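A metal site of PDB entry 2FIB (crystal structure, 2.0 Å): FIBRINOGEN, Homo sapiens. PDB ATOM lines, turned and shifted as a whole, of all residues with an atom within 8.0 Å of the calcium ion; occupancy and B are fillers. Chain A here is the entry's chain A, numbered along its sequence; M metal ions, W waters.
The calcium ion is bound by O of Phe 180. The calcium ion is bound by O of Gly 182 (2.3 Å). The calcium ion is bound by OD2 of Asp 176. The side-chain carboxylate (OD1) of Asp 178 binds the calcium ion (2.4 Å). The calcium ion is bound by water W1 (2.5 Å). The calcium ion is bound by water W2, at 2.5 Å. The calcium ion has six donor atoms within binding distance. Slightly farther from the calcium ion lies OD1 of Asp 176 (3.0 Å).
Water W2 bridges the backbone carbonyl oxygen of Asp 178 (2.6 Å) and the side-chain carboxylate of Asp 176 (3.4 Å).
C of Glu 181 touches the calcium ion (3.96 Å).
The backbone NH (N) of Asp 178 is in hydrogen-bond range of the side-chain hydroxyl (OG) of Ser 171 (3.3 Å). OD2 of Asp 178 is in hydrogen-bond range of N of Cys 184 (2.9 Å).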
ATOM      1  N   SER A 171      26.072 -18.569 -27.471  1.00  0.00           N
ATOM      2  CA  SER A 171      24.924 -19.178 -28.141  1.00  0.00           C
ATOM      3  C   SER A 171      23.669 -18.295 -28.029  1.00  0.00           C
ATOM      4  O   SER A 171      23.389 -17.751 -26.953  1.00  0.00           O
ATOM      5  CB  SER A 171      24.552 -20.513 -27.490  1.00  0.00           C
ATOM      6  OG  SER A 171      25.583 -21.477 -27.526  1.00  0.00           O
ATOM      7  N   ASN A 175      21.776 -19.596 -33.021  1.00  0.00           N
ATOM      8  CA  ASN A 175      23.190 -19.843 -33.263  1.00  0.00           C
ATOM      9  C   ASN A 175      23.624 -20.640 -32.081  1.00  0.00           C
ATOM     10  O   ASN A 175      24.107 -20.106 -31.081  1.00  0.00           O
ATOM     11  CB  ASN A 175      23.995 -18.540 -33.372  1.00  0.00           C
ATOM     12  CG  ASN A 175      25.099 -18.649 -34.403  1.00  0.00           C
ATOM     13  OD1 ASN A 175      25.885 -19.597 -34.404  1.00  0.00           O
ATOM     14  ND2 ASN A 175      25.138 -17.700 -35.330  1.00  0.00           N
ATOM     15  N   ASP A 176      23.294 -21.917 -32.168  1.00  0.00           N
ATOM     16  CA  ASP A 176      23.563 -22.883 -31.117  1.00  0.00           C
ATOM     17  C   ASP A 176      24.969 -23.437 -31.162  1.00  0.00           C
ATOM     18  O   ASP A 176      25.289 -24.274 -32.005  1.00  0.00           O
ATOM     19  CB  ASP A 176      22.538 -24.010 -31.225  1.00  0.00           C
ATOM     20  CG  ASP A 176      22.679 -25.035 -30.144  1.00  0.00           C
ATOM     21  OD1 ASP A 176      23.600 -24.971 -29.312  1.00  0.00           O
ATOM     22  OD2 ASP A 176      21.843 -25.934 -30.113  1.00  0.00           O
ATOM     23  N   ASN A 177      25.745 -23.076 -30.159  1.00  0.00           N
ATOM     24  CA  ASN A 177      27.123 -23.532 -30.085  1.00  0.00           C
ATOM     25  C   ASN A 177      27.365 -24.144 -28.711  1.00  0.00           C
ATOM     26  O   ASN A 177      28.491 -24.203 -28.254  1.00  0.00           O
ATOM     27  CB  ASN A 177      28.078 -22.341 -30.321  1.00  0.00           C
ATOM     28  CG  ASN A 177      27.805 -21.604 -31.634  1.00  0.00           C
ATOM     29  OD1 ASN A 177      28.068 -22.117 -32.718  1.00  0.00           O
ATOM     30  ND2 ASN A 177      27.284 -20.387 -31.530  1.00  0.00           N
ATOM     31  N   ASP A 178      26.292 -24.615 -28.058  1.00  0.00           N
ATOM     32  CA  ASP A 178      26.439 -25.227 -26.735  1.00  0.00           C
ATOM     33  C   ASP A 178      26.879 -26.692 -26.767  1.00  0.00           C
ATOM     34  O   ASP A 178      27.188 -27.219 -27.827  1.00  0.00           O
ATOM     35  CB  ASP A 178      25.185 -25.024 -25.852  1.00  0.00           C
ATOM     36  CG  ASP A 178      23.942 -25.779 -26.368  1.00  0.00           C
ATOM     37  OD1 ASP A 178      24.059 -26.735 -27.157  1.00  0.00           O
ATOM     38  OD2 ASP A 178      22.818 -25.414 -25.947  1.00  0.00           O
ATOM     39  N   LYS A 179      26.871 -27.328 -25.606  1.00  0.00           N
ATOM     40  CA  LYS A 179      27.275 -28.723 -25.461  1.00  0.00           C
ATOM     41  C   LYS A 179      26.067 -29.648 -25.172  1.00  0.00           C
ATOM     42  O   LYS A 179      26.230 -30.780 -24.709  1.00  0.00           O
ATOM     43  CB  LYS A 179      28.283 -28.832 -24.314  1.00  0.00           C
ATOM     44  CG  LYS A 179      29.610 -28.076 -24.569  1.00  0.00           C
ATOM     45  CD  LYS A 179      30.768 -29.044 -24.855  1.00  0.00           C
ATOM     46  CE  LYS A 179      32.036 -28.311 -25.322  1.00  0.00           C
ATOM     47  NZ  LYS A 179      31.843 -27.674 -26.667  1.00  0.00           N
ATOM     48  N   PHE A 180      24.874 -29.145 -25.442  1.00  0.00           N
ATOM     49  CA  PHE A 180      23.621 -29.863 -25.194  1.00  0.00           C
ATOM     50  C   PHE A 180      23.014 -30.208 -26.541  1.00  0.00           C
ATOM     51  O   PHE A 180      23.085 -29.394 -27.451  1.00  0.00           O
ATOM     52  CB  PHE A 180      22.678 -28.925 -24.402  1.00  0.00           C
ATOM     53  CG  PHE A 180      21.302 -29.485 -24.159  1.00  0.00           C
ATOM     54  CD1 PHE A 180      21.128 -30.753 -23.630  1.00  0.00           C
ATOM     55  CD2 PHE A 180      20.174 -28.702 -24.430  1.00  0.00           C
ATOM     56  CE1 PHE A 180      19.845 -31.249 -23.370  1.00  0.00           C
ATOM     57  CE2 PHE A 180      18.912 -29.188 -24.176  1.00  0.00           C
ATOM     58  CZ  PHE A 180      18.738 -30.456 -23.646  1.00  0.00           C
ATOM     59  N   GLU A 181      22.393 -31.387 -26.681  1.00  0.00           N
ATOM     60  CA  GLU A 181      21.822 -31.729 -27.983  1.00  0.00           C
ATOM     61  C   GLU A 181      20.535 -30.985 -28.296  1.00  0.00           C
ATOM     62  O   GLU A 181      19.982 -31.122 -29.389  1.00  0.00           O
ATOM     63  CB  GLU A 181      21.632 -33.212 -28.160  1.00  0.00           C
ATOM     64  CG  GLU A 181      22.593 -34.040 -27.387  1.00  0.00           C
ATOM     65  CD  GLU A 181      21.853 -34.703 -26.273  1.00  0.00           C
ATOM     66  OE1 GLU A 181      21.311 -35.807 -26.547  1.00  0.00           O
ATOM     67  OE2 GLU A 181      21.784 -34.100 -25.166  1.00  0.00           O
ATOM     68  N   GLY A 182      20.024 -30.249 -27.315  1.00  0.00           N
ATOM     69  CA  GLY A 182      18.865 -29.408 -27.552  1.00  0.00           C
ATOM     70  C   GLY A 182      19.454 -28.015 -27.755  1.00  0.00           C
ATOM     71  O   GLY A 182      20.660 -27.866 -28.035  1.00  0.00           O
ATOM     72  N   ASN A 183      18.649 -26.980 -27.634  1.00  0.00           N
ATOM     73  CA  ASN A 183      19.189 -25.641 -27.789  1.00  0.00           C
ATOM     74  C   ASN A 183      18.941 -24.926 -26.466  1.00  0.00           C
ATOM     75  O   ASN A 183      17.784 -24.628 -26.149  1.00  0.00           O
ATOM     76  CB  ASN A 183      18.497 -24.917 -28.949  1.00  0.00           C
ATOM     77  CG  ASN A 183      19.124 -23.545 -29.242  1.00  0.00           C
ATOM     78  OD1 ASN A 183      19.737 -22.928 -28.379  1.00  0.00           O
ATOM     79  ND2 ASN A 183      18.950 -23.074 -30.473  1.00  0.00           N
ATOM     80  N   CYS A 184      20.002 -24.733 -25.663  1.00  0.00           N
ATOM     81  CA  CYS A 184      19.904 -24.074 -24.350  1.00  0.00           C
ATOM     82  C   CYS A 184      19.419 -22.629 -24.468  1.00  0.00           C
ATOM     83  O   CYS A 184      18.518 -22.206 -23.762  1.00  0.00           O
ATOM     84  CB  CYS A 184      21.252 -23.992 -23.638  1.00  0.00           C
ATOM     85  SG  CYS A 184      21.994 -25.534 -23.056  1.00  0.00           S
ATOM     86  N   ALA A 185      20.095 -21.875 -25.325  1.00  0.00           N
ATOM     87  CA  ALA A 185      19.767 -20.477 -25.522  1.00  0.00           C
ATOM     88  C   ALA A 185      18.299 -20.377 -25.871  1.00  0.00           C
ATOM     89  O   ALA A 185      17.566 -19.618 -25.248  1.00  0.00           O
ATOM     90  CB  ALA A 185      20.621 -19.902 -26.613  1.00  0.00           C
ATOM     91  N   MET A 194      26.613 -20.756 -23.127  1.00  0.00           N
ATOM     92  CA  MET A 194      25.997 -22.014 -22.697  1.00  0.00           C
ATOM     93  C   MET A 194      26.871 -23.264 -22.816  1.00  0.00           C
ATOM     94  O   MET A 194      27.554 -23.460 -23.814  1.00  0.00           O
ATOM     95  CB  MET A 194      24.723 -22.315 -23.538  1.00  0.00           C
ATOM     96  CG  MET A 194      23.621 -21.283 -23.462  1.00  0.00           C
ATOM     97  SD  MET A 194      23.000 -21.010 -21.788  1.00  0.00           S
ATOM     98  CE  MET A 194      21.413 -20.195 -22.178  1.00  0.00           C
ATOM     99  N   ASN A 195      26.758 -24.128 -21.816  1.00  0.00           N
ATOM    100  CA  ASN A 195      27.439 -25.432 -21.760  1.00  0.00           C
ATOM    101  C   ASN A 195      26.243 -26.399 -21.880  1.00  0.00           C
ATOM    102  O   ASN A 195      25.676 -26.577 -22.959  1.00  0.00           O
ATOM    103  CB  ASN A 195      28.179 -25.616 -20.410  1.00  0.00           C
ATOM    104  CG  ASN A 195      29.064 -26.877 -20.355  1.00  0.00           C
ATOM    105  OD1 ASN A 195      29.039 -27.702 -21.267  1.00  0.00           O
ATOM    106  ND2 ASN A 195      29.858 -27.018 -19.298  1.00  0.00           N
HETATM  107 CA    CA M   1      22.806 -27.799 -28.936  1.00  0.00          CA
HETATM  108  O   HOH W   1      22.403 -28.886 -31.128  1.00  0.00           O
HETATM  109  O   HOH W   2      25.280 -27.897 -29.505  1.00  0.00           O
